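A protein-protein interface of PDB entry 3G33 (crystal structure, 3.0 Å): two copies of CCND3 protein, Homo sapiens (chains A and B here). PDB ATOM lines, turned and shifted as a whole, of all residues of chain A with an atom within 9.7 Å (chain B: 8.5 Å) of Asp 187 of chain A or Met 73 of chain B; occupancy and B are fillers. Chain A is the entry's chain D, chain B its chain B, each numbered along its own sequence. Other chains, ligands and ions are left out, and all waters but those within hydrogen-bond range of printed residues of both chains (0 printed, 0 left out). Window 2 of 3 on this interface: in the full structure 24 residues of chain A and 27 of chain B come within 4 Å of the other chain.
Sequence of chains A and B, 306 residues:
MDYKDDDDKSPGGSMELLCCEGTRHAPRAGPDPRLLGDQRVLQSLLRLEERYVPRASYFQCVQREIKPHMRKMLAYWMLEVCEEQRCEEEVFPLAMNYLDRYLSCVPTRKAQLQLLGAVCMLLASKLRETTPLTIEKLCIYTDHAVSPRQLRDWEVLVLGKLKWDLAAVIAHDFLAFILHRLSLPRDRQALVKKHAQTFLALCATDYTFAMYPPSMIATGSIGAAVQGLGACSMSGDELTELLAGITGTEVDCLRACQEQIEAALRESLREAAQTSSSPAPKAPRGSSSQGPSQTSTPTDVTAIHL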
ATOM      1  N   LEU A 179      13.912 -22.621  32.811  1.00  0.00           N
ATOM      2  CA  LEU A 179      13.024 -22.009  31.831  1.00  0.00           C
ATOM      3  C   LEU A 179      12.023 -23.036  31.315  1.00  0.00           C
ATOM      4  O   LEU A 179      10.848 -22.729  31.126  1.00  0.00           O
ATOM      5  CB  LEU A 179      13.819 -21.407  30.669  1.00  0.00           C
ATOM      6  CG  LEU A 179      14.436 -20.029  30.912  1.00  0.00           C
ATOM      7  CD1 LEU A 179      15.302 -19.612  29.735  1.00  0.00           C
ATOM      8  CD2 LEU A 179      13.352 -18.995  31.175  1.00  0.00           C
ATOM      9  N   SER A 183       5.728 -21.705  32.834  1.00  0.00           N
ATOM     10  CA  SER A 183       4.443 -21.663  32.161  1.00  0.00           C
ATOM     11  C   SER A 183       4.574 -20.848  30.885  1.00  0.00           C
ATOM     12  O   SER A 183       3.610 -20.241  30.415  1.00  0.00           O
ATOM     13  CB  SER A 183       3.387 -21.043  33.076  1.00  0.00           C
ATOM     14  OG  SER A 183       3.785 -19.754  33.509  1.00  0.00           O
ATOM     15  N   LEU A 184       5.782 -20.836  30.333  1.00  0.00           N
ATOM     16  CA  LEU A 184       6.060 -20.104  29.107  1.00  0.00           C
ATOM     17  C   LEU A 184       6.409 -21.052  27.969  1.00  0.00           C
ATOM     18  O   LEU A 184       7.010 -22.105  28.189  1.00  0.00           O
ATOM     19  CB  LEU A 184       7.206 -19.112  29.322  1.00  0.00           C
ATOM     20  CG  LEU A 184       6.980 -18.015  30.364  1.00  0.00           C
ATOM     21  CD1 LEU A 184       8.193 -17.101  30.443  1.00  0.00           C
ATOM     22  CD2 LEU A 184       5.723 -17.219  30.045  1.00  0.00           C
ATOM     23  N   PRO A 185       6.026 -20.673  26.743  1.00  0.00           N
ATOM     24  CA  PRO A 185       6.337 -21.383  25.511  1.00  0.00           C
ATOM     25  C   PRO A 185       7.678 -20.938  24.937  1.00  0.00           C
ATOM     26  O   PRO A 185       8.086 -19.792  25.134  1.00  0.00           O
ATOM     27  CB  PRO A 185       5.203 -20.959  24.574  1.00  0.00           C
ATOM     28  CG  PRO A 185       4.780 -19.610  25.067  1.00  0.00           C
ATOM     29  CD  PRO A 185       5.201 -19.475  26.507  1.00  0.00           C
ATOM     30  N   ARG A 186       8.362 -21.842  24.242  1.00  0.00           N
ATOM     31  CA  ARG A 186       9.598 -21.492  23.554  1.00  0.00           C
ATOM     32  C   ARG A 186       9.335 -20.371  22.556  1.00  0.00           C
ATOM     33  O   ARG A 186      10.265 -19.746  22.046  1.00  0.00           O
ATOM     34  CB  ARG A 186      10.173 -22.708  22.824  1.00  0.00           C
ATOM     35  CG  ARG A 186      10.915 -23.690  23.713  1.00  0.00           C
ATOM     36  CD  ARG A 186      11.497 -24.830  22.888  1.00  0.00           C
ATOM     37  NE  ARG A 186      12.456 -25.632  23.644  1.00  0.00           N
ATOM     38  CZ  ARG A 186      13.104 -26.681  23.151  1.00  0.00           C
ATOM     39  NH1 ARG A 186      12.896 -27.062  21.897  1.00  0.00           N
ATOM     40  NH2 ARG A 186      13.960 -27.352  23.910  1.00  0.00           N
ATOM     41  N   ASP A 187       8.059 -20.123  22.281  1.00  0.00           N
ATOM     42  CA  ASP A 187       7.665 -19.109  21.313  1.00  0.00           C
ATOM     43  C   ASP A 187       8.062 -17.705  21.764  1.00  0.00           C
ATOM     44  O   ASP A 187       8.188 -16.796  20.943  1.00  0.00           O
ATOM     45  CB  ASP A 187       6.157 -19.170  21.060  1.00  0.00           C
ATOM     46  CG  ASP A 187       5.694 -20.548  20.630  1.00  0.00           C
ATOM     47  OD1 ASP A 187       6.506 -21.495  20.703  1.00  0.00           O
ATOM     48  OD2 ASP A 187       4.521 -20.684  20.224  1.00  0.00           O
ATOM     49  N   ARG A 188       8.261 -17.533  23.067  1.00  0.00           N
ATOM     50  CA  ARG A 188       8.600 -16.224  23.620  1.00  0.00           C
ATOM     51  C   ARG A 188       9.873 -16.253  24.460  1.00  0.00           C
ATOM     52  O   ARG A 188      10.284 -15.229  25.006  1.00  0.00           O
ATOM     53  CB  ARG A 188       7.444 -15.684  24.467  1.00  0.00           C
ATOM     54  CG  ARG A 188       6.202 -15.291  23.680  1.00  0.00           C
ATOM     55  CD  ARG A 188       5.151 -14.691  24.604  1.00  0.00           C
ATOM     56  NE  ARG A 188       3.932 -14.316  23.896  1.00  0.00           N
ATOM     57  CZ  ARG A 188       2.851 -13.817  24.487  1.00  0.00           C
ATOM     58  NH1 ARG A 188       2.838 -13.633  25.801  1.00  0.00           N
ATOM     59  NH2 ARG A 188       1.782 -13.503  23.767  1.00  0.00           N
ATOM     60  N   GLN A 189      10.496 -17.423  24.562  1.00  0.00           N
ATOM     61  CA  GLN A 189      11.671 -17.593  25.417  1.00  0.00           C
ATOM     62  C   GLN A 189      12.872 -16.753  24.984  1.00  0.00           C
ATOM     63  O   GLN A 189      13.774 -16.494  25.781  1.00  0.00           O
ATOM     64  CB  GLN A 189      12.075 -19.067  25.496  1.00  0.00           C
ATOM     65  CG  GLN A 189      11.208 -19.907  26.418  1.00  0.00           C
ATOM     66  CD  GLN A 189      11.928 -21.148  26.914  1.00  0.00           C
ATOM     67  OE1 GLN A 189      13.154 -21.242  26.837  1.00  0.00           O
ATOM     68  NE2 GLN A 189      11.167 -22.106  27.431  1.00  0.00           N
ATOM     69  N   ALA A 190      12.882 -16.333  23.724  1.00  0.00           N
ATOM     70  CA  ALA A 190      14.012 -15.590  23.173  1.00  0.00           C
ATOM     71  C   ALA A 190      14.341 -14.332  23.978  1.00  0.00           C
ATOM     72  O   ALA A 190      15.468 -14.166  24.448  1.00  0.00           O
ATOM     73  CB  ALA A 190      13.756 -15.240  21.713  1.00  0.00           C
ATOM     74  N   LEU A 191      13.357 -13.451  24.131  1.00  0.00           N
ATOM     75  CA  LEU A 191      13.561 -12.187  24.835  1.00  0.00           C
ATOM     76  C   LEU A 191      13.832 -12.368  26.325  1.00  0.00           C
ATOM     77  O   LEU A 191      14.720 -11.725  26.883  1.00  0.00           O
ATOM     78  CB  LEU A 191      12.370 -11.248  24.632  1.00  0.00           C
ATOM     79  CG  LEU A 191      12.541 -10.189  23.542  1.00  0.00           C
ATOM     80  CD1 LEU A 191      11.272  -9.367  23.389  1.00  0.00           C
ATOM     81  CD2 LEU A 191      13.729  -9.294  23.862  1.00  0.00           C
ATOM     82  N   VAL A 192      13.061 -13.239  26.967  1.00  0.00           N
ATOM     83  CA  VAL A 192      13.238 -13.491  28.391  1.00  0.00           C
ATOM     84  C   VAL A 192      14.665 -13.945  28.682  1.00  0.00           C
ATOM     85  O   VAL A 192      15.325 -13.424  29.580  1.00  0.00           O
ATOM     86  CB  VAL A 192      12.258 -14.561  28.901  1.00  0.00           C
ATOM     87  CG1 VAL A 192      12.475 -14.811  30.386  1.00  0.00           C
ATOM     88  CG2 VAL A 192      10.824 -14.140  28.631  1.00  0.00           C
ATOM     89  N   LYS B  67      -0.696 -12.800   9.499  1.00  0.00           N
ATOM     90  CA  LYS B  67      -1.283 -12.066  10.591  1.00  0.00           C
ATOM     91  C   LYS B  67      -0.230 -11.569  11.547  1.00  0.00           C
ATOM     92  O   LYS B  67       0.817 -12.191  11.715  1.00  0.00           O
ATOM     93  CB  LYS B  67      -2.381 -12.882  11.277  1.00  0.00           C
ATOM     94  CG  LYS B  67      -3.578 -13.133  10.363  1.00  0.00           C
ATOM     95  CD  LYS B  67      -4.788 -13.636  11.128  1.00  0.00           C
ATOM     96  CE  LYS B  67      -5.988 -13.816  10.209  1.00  0.00           C
ATOM     97  NZ  LYS B  67      -7.189 -14.277  10.958  1.00  0.00           N
ATOM     98  N   PRO B  68      -0.497 -10.410  12.152  1.00  0.00           N
ATOM     99  CA  PRO B  68       0.465  -9.756  13.021  1.00  0.00           C
ATOM    100  C   PRO B  68       1.072 -10.730  14.029  1.00  0.00           C
ATOM    101  O   PRO B  68       2.264 -10.644  14.322  1.00  0.00           O
ATOM    102  CB  PRO B  68      -0.372  -8.693  13.737  1.00  0.00           C
ATOM    103  CG  PRO B  68      -1.498  -8.402  12.799  1.00  0.00           C
ATOM    104  CD  PRO B  68      -1.761  -9.662  12.032  1.00  0.00           C
ATOM    105  N   HIS B  69       0.267 -11.649  14.554  1.00  0.00           N
ATOM    106  CA  HIS B  69       0.765 -12.595  15.551  1.00  0.00           C
ATOM    107  C   HIS B  69       1.789 -13.559  14.956  1.00  0.00           C
ATOM    108  O   HIS B  69       2.729 -13.973  15.632  1.00  0.00           O
ATOM    109  CB  HIS B  69      -0.381 -13.365  16.215  1.00  0.00           C
ATOM    110  CG  HIS B  69      -1.164 -14.225  15.271  1.00  0.00           C
ATOM    111  ND1 HIS B  69      -2.327 -13.798  14.668  1.00  0.00           N
ATOM    112  CD2 HIS B  69      -0.958 -15.490  14.835  1.00  0.00           C
ATOM    113  CE1 HIS B  69      -2.801 -14.760  13.897  1.00  0.00           C
ATOM    114  NE2 HIS B  69      -1.989 -15.799  13.980  1.00  0.00           N
ATOM    115  N   MET B  70       1.603 -13.908  13.687  1.00  0.00           N
ATOM    116  CA  MET B  70       2.533 -14.793  12.995  1.00  0.00           C
ATOM    117  C   MET B  70       3.853 -14.080  12.720  1.00  0.00           C
ATOM    118  O   MET B  70       4.917 -14.698  12.722  1.00  0.00           O
ATOM    119  CB  MET B  70       1.923 -15.295  11.686  1.00  0.00           C
ATOM    120  CG  MET B  70       0.670 -16.137  11.868  1.00  0.00           C
ATOM    121  SD  MET B  70      -0.156 -16.512  10.309  1.00  0.00           S
ATOM    122  CE  MET B  70       1.138 -17.390   9.437  1.00  0.00           C
ATOM    123  N   ARG B  71       3.775 -12.775  12.483  1.00  0.00           N
ATOM    124  CA  ARG B  71       4.957 -11.967  12.218  1.00  0.00           C
ATOM    125  C   ARG B  71       5.827 -11.871  13.465  1.00  0.00           C
ATOM    126  O   ARG B  71       7.052 -11.800  13.378  1.00  0.00           O
ATOM    127  CB  ARG B  71       4.547 -10.571  11.741  1.00  0.00           C
ATOM    128  CG  ARG B  71       5.699  -9.688  11.284  1.00  0.00           C
ATOM    129  CD  ARG B  71       6.295  -8.903  12.439  1.00  0.00           C
ATOM    130  NE  ARG B  71       7.266  -7.914  11.979  1.00  0.00           N
ATOM    131  CZ  ARG B  71       7.918  -7.078  12.781  1.00  0.00           C
ATOM    132  NH1 ARG B  71       7.706  -7.110  14.090  1.00  0.00           N
ATOM    133  NH2 ARG B  71       8.786  -6.213  12.275  1.00  0.00           N
ATOM    134  N   LYS B  72       5.182 -11.877  14.626  1.00  0.00           N
ATOM    135  CA  LYS B  72       5.891 -11.833  15.897  1.00  0.00           C
ATOM    136  C   LYS B  72       6.367 -13.225  16.299  1.00  0.00           C
ATOM    137  O   LYS B  72       7.463 -13.385  16.836  1.00  0.00           O
ATOM    138  CB  LYS B  72       4.998 -11.230  16.981  1.00  0.00           C
ATOM    139  CG  LYS B  72       4.562  -9.804  16.676  1.00  0.00           C
ATOM    140  CD  LYS B  72       3.350  -9.394  17.496  1.00  0.00           C
ATOM    141  CE  LYS B  72       2.832  -8.033  17.057  1.00  0.00           C
ATOM    142  NZ  LYS B  72       1.558  -7.674  17.740  1.00  0.00           N
ATOM    143  N   MET B  73       5.540 -14.231  16.030  1.00  0.00           N
ATOM    144  CA  MET B  73       5.916 -15.617  16.284  1.00  0.00           C
ATOM    145  C   MET B  73       7.171 -15.983  15.503  1.00  0.00           C
ATOM    146  O   MET B  73       8.014 -16.742  15.980  1.00  0.00           O
ATOM    147  CB  MET B  73       4.773 -16.563  15.914  1.00  0.00           C
ATOM    148  CG  MET B  73       3.702 -16.690  16.984  1.00  0.00           C
ATOM    149  SD  MET B  73       4.319 -17.488  18.481  1.00  0.00           S
ATOM    150  CE  MET B  73       4.810 -19.086  17.836  1.00  0.00           C
ATOM    151  N   LEU B  74       7.287 -15.439  14.297  1.00  0.00           N
ATOM    152  CA  LEU B  74       8.459 -15.672  13.464  1.00  0.00           C
ATOM    153  C   LEU B  74       9.649 -14.887  14.000  1.00  0.00           C
ATOM    154  O   LEU B  74      10.792 -15.334  13.914  1.00  0.00           O
ATOM    155  CB  LEU B  74       8.172 -15.264  12.018  1.00  0.00           C
ATOM    156  CG  LEU B  74       9.295 -15.491  11.005  1.00  0.00           C
ATOM    157  CD1 LEU B  74       9.556 -16.976  10.820  1.00  0.00           C
ATOM    158  CD2 LEU B  74       8.953 -14.839   9.677  1.00  0.00           C
ATOM    159  N   ALA B  75       9.370 -13.712  14.558  1.00  0.00           N
ATOM    160  CA  ALA B  75      10.417 -12.837  15.072  1.00  0.00           C
ATOM    161  C   ALA B  75      11.192 -13.492  16.211  1.00  0.00           C
ATOM    162  O   ALA B  75      12.416 -13.388  16.281  1.00  0.00           O
ATOM    163  CB  ALA B  75       9.822 -11.513  15.527  1.00  0.00           C
ATOM    164  N   TYR B  76      10.474 -14.166  17.103  1.00  0.00           N
ATOM    165  CA  TYR B  76      11.104 -14.828  18.237  1.00  0.00           C
ATOM    166  C   TYR B  76      11.948 -16.019  17.797  1.00  0.00           C
ATOM    167  O   TYR B  76      12.935 -16.363  18.445  1.00  0.00           O
ATOM    168  CB  TYR B  76      10.055 -15.260  19.263  1.00  0.00           C
ATOM    169  CG  TYR B  76       9.578 -14.130  20.146  1.00  0.00           C
ATOM    170  CD1 TYR B  76       8.505 -13.335  19.770  1.00  0.00           C
ATOM    171  CD2 TYR B  76      10.205 -13.857  21.355  1.00  0.00           C
ATOM    172  CE1 TYR B  76       8.068 -12.299  20.576  1.00  0.00           C
ATOM    173  CE2 TYR B  76       9.774 -12.825  22.165  1.00  0.00           C
ATOM    174  CZ  TYR B  76       8.706 -12.049  21.773  1.00  0.00           C
ATOM    175  OH  TYR B  76       8.275 -11.020  22.577  1.00  0.00           O
ATOM    176  N   TRP B  77      11.557 -16.645  16.693  1.00  0.00           N
ATOM    177  CA  TRP B  77      12.329 -17.753  16.148  1.00  0.00           C
ATOM    178  C   TRP B  77      13.626 -17.244  15.530  1.00  0.00           C
ATOM    179  O   TRP B  77      14.663 -17.904  15.610  1.00  0.00           O
ATOM    180  CB  TRP B  77      11.515 -18.532  15.113  1.00  0.00           C
ATOM    181  CG  TRP B  77      12.299 -19.624  14.455  1.00  0.00           C
ATOM    182  CD1 TRP B  77      12.658 -20.821  15.003  1.00  0.00           C
ATOM    183  CD2 TRP B  77      12.826 -19.618  13.123  1.00  0.00           C
ATOM    184  NE1 TRP B  77      13.376 -21.561  14.095  1.00  0.00           N
ATOM    185  CE2 TRP B  77      13.493 -20.845  12.932  1.00  0.00           C
ATOM    186  CE3 TRP B  77      12.798 -18.696  12.074  1.00  0.00           C
ATOM    187  CZ2 TRP B  77      14.125 -21.173  11.735  1.00  0.00           C
ATOM    188  CZ3 TRP B  77      13.427 -19.023  10.886  1.00  0.00           C
ATOM    189  CH2 TRP B  77      14.081 -20.249  10.727  1.00  0.00           C
ATOM    190  N   MET B  78      13.563 -16.069  14.913  1.00  0.00           N
ATOM    191  CA  MET B  78      14.755 -15.442  14.355  1.00  0.00           C
ATOM    192  C   MET B  78      15.690 -15.013  15.479  1.00  0.00           C
ATOM    193  O   MET B  78      16.912 -15.083  15.345  1.00  0.00           O
ATOM    194  CB  MET B  78      14.383 -14.235  13.493  1.00  0.00           C
ATOM    195  CG  MET B  78      13.508 -14.562  12.294  1.00  0.00           C
ATOM    196  SD  MET B  78      13.470 -13.224  11.081  1.00  0.00           S
ATOM    197  CE  MET B  78      12.145 -13.770  10.010  1.00  0.00           C
ATOM    198  N   LEU B  79      15.107 -14.572  16.589  1.00  0.00           N
ATOM    199  CA  LEU B  79      15.885 -14.149  17.743  1.00  0.00           C
ATOM    200  C   LEU B  79      16.609 -15.341  18.365  1.00  0.00           C
ATOM    201  O   LEU B  79      17.780 -15.246  18.733  1.00  0.00           O
ATOM    202  CB  LEU B  79      14.983 -13.475  18.778  1.00  0.00           C
ATOM    203  CG  LEU B  79      15.686 -12.725  19.908  1.00  0.00           C
ATOM    204  CD1 LEU B  79      16.561 -11.614  19.347  1.00  0.00           C
ATOM    205  CD2 LEU B  79      14.670 -12.168  20.895  1.00  0.00           C
ATOM    206  N   GLU B  80      15.905 -16.463  18.479  1.00  0.00           N
ATOM    207  CA  GLU B  80      16.504 -17.682  19.005  1.00  0.00           C
ATOM    208  C   GLU B  80      17.708 -18.096  18.173  1.00  0.00           C
ATOM    209  O   GLU B  80      18.769 -18.410  18.711  1.00  0.00           O
ATOM    210  CB  GLU B  80      15.487 -18.825  19.033  1.00  0.00           C
ATOM    211  CG  GLU B  80      14.697 -18.934  20.324  1.00  0.00           C
ATOM    212  CD  GLU B  80      14.058 -20.298  20.489  1.00  0.00           C
ATOM    213  OE1 GLU B  80      14.101 -21.092  19.525  1.00  0.00           O
ATOM    214  OE2 GLU B  80      13.517 -20.577  21.581  1.00  0.00           O
ATOM    215  N   MET B  96      14.824  -8.480  10.225  1.00  0.00           N
ATOM    216  CA  MET B  96      13.438  -8.053  10.365  1.00  0.00           C
ATOM    217  C   MET B  96      13.145  -6.879   9.442  1.00  0.00           C
ATOM    218  O   MET B  96      12.029  -6.729   8.946  1.00  0.00           O
ATOM    219  CB  MET B  96      13.128  -7.684  11.816  1.00  0.00           C
ATOM    220  CG  MET B  96      13.123  -8.872  12.760  1.00  0.00           C
ATOM    221  SD  MET B  96      12.016 -10.179  12.198  1.00  0.00           S
ATOM    222  CE  MET B  96      10.434  -9.343  12.277  1.00  0.00           C
ATOM    223  N   LEU B  99      12.489  -8.418   6.172  1.00  0.00           N
ATOM    224  CA  LEU B  99      11.178  -9.051   6.239  1.00  0.00           C
ATOM    225  C   LEU B  99      10.063  -8.052   5.945  1.00  0.00           C
ATOM    226  O   LEU B  99       9.288  -8.231   5.005  1.00  0.00           O
ATOM    227  CB  LEU B  99      10.962  -9.693   7.611  1.00  0.00           C
ATOM    228  CG  LEU B  99       9.666 -10.486   7.787  1.00  0.00           C
ATOM    229  CD1 LEU B  99       9.687 -11.747   6.935  1.00  0.00           C
ATOM    230  CD2 LEU B  99       9.445 -10.831   9.250  1.00  0.00           C
ATOM    231  N   LEU B 113       6.426 -18.657   4.999  1.00  0.00           N
ATOM    232  CA  LEU B 113       6.867 -17.669   5.976  1.00  0.00           C
ATOM    233  C   LEU B 113       8.215 -18.033   6.592  1.00  0.00           C
ATOM    234  O   LEU B 113       9.126 -17.207   6.644  1.00  0.00           O
ATOM    235  CB  LEU B 113       5.814 -17.491   7.071  1.00  0.00           C
ATOM    236  CG  LEU B 113       5.971 -16.271   7.980  1.00  0.00           C
ATOM    237  CD1 LEU B 113       6.058 -14.995   7.156  1.00  0.00           C
ATOM    238  CD2 LEU B 113       4.823 -16.196   8.974  1.00  0.00           C
ATOM    239  N   THR B 205      10.846  -7.236  17.483  1.00  0.00           N
ATOM    240  CA  THR B 205       9.858  -8.302  17.582  1.00  0.00           C
ATOM    241  C   THR B 205       8.442  -7.740  17.578  1.00  0.00           C
ATOM    242  O   THR B 205       7.510  -8.383  17.094  1.00  0.00           O
ATOM    243  CB  THR B 205      10.064  -9.153  18.853  1.00  0.00           C
ATOM    244  OG1 THR B 205       9.829  -8.350  20.017  1.00  0.00           O
ATOM    245  CG2 THR B 205      11.480  -9.710  18.902  1.00  0.00           C
ATOM    246  N   ASP B 206       8.291  -6.534  18.115  1.00  0.00           N
ATOM    247  CA  ASP B 206       6.982  -5.906  18.240  1.00  0.00           C
ATOM    248  C   ASP B 206       6.663  -5.037  17.023  1.00  0.00           C
ATOM    249  O   ASP B 206       7.384  -4.086  16.720  1.00  0.00           O
ATOM    250  CB  ASP B 206       6.922  -5.072  19.520  1.00  0.00           C
ATOM    251  CG  ASP B 206       5.507  -4.868  20.015  1.00  0.00           C
ATOM    252  OD1 ASP B 206       4.588  -4.759  19.177  1.00  0.00           O
ATOM    253  OD2 ASP B 206       5.316  -4.814  21.249  1.00  0.00           O
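The guanidinium group of Arg 71 of chain B sits at hydrogen-bond distance from the backbone carbonyl oxygen of Thr 205 of chain B (3.3 Å).
No position is printed for both chains.
Of the 19 printed residues of chain B, 5 touch a printed residue of chain A.
Hydrophobic or aromatic side chains of chain B within 4 Å of the printed part of chain A: Met 73, Tyr 76 and Leu 79.
Among the printed residues, no Asp or Glu carboxylate lies within 4 Å of a Lys or Arg side-chain nitrogen of the other chain.
OE2 of Glu 80 of chain B sits close to O of Arg 186 of chain A (3.4 Å).
The side-chain carboxylate (OD2) of Asp 187 of chain A lies close to the side-chain sulfur (SD) of Met 73 of chain B, at 3.6 Å.
Of chain B, only Met 73 and Tyr 76 come within 4 Å of Asp 187 of chain A.
Of chain A, only Asp 187 (2.9 Å) comes within 4 Å of Met 73 of chain B.
No residue of chain A comes within 4 Å of Ala 75 of chain B.
Of the printed residues of chain B, Leu 191 of chain A touches Tyr 76 (3.5 Å), Leu 79 (3.7 Å) and Thr 205 (3.8 Å).
Printed residues of chain A within 4 Å of Glu 80 of chain B: Arg 186.
Of the printed residues of chain A, Leu 79 of chain B touches Ala 190 (3.3 Å) and Leu 191 (3.7 Å).
Printed residues of chain B within 4 Å of Arg 188 of chain A: Tyr 76.
Lys 67 of chain B touches none of the printed residues of chain A.
The nearest residue of chain B that does not touch Asp 187 of chain A is Lys 72 of chain B (5.4 Å).
Among the printed residues, pairs that only touch across the chains: Asp 187 of chain A with Tyr 76 of chain B (2.9 Å), Arg 188 of chain A with Tyr 76 of chain B (3.6 Å), Ala 190 of chain A with Tyr 76 of chain B (3.6 Å), Ala 190 of chain A with Leu 79 of chain B (3.3 Å), Leu 191 of chain A with Tyr 76 of chain B (3.5 Å), Leu 191 of chain A with Leu 79 of chain B (3.7 Å) and Leu 191 of chain A with Thr 205 of chain B (3.8 Å).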
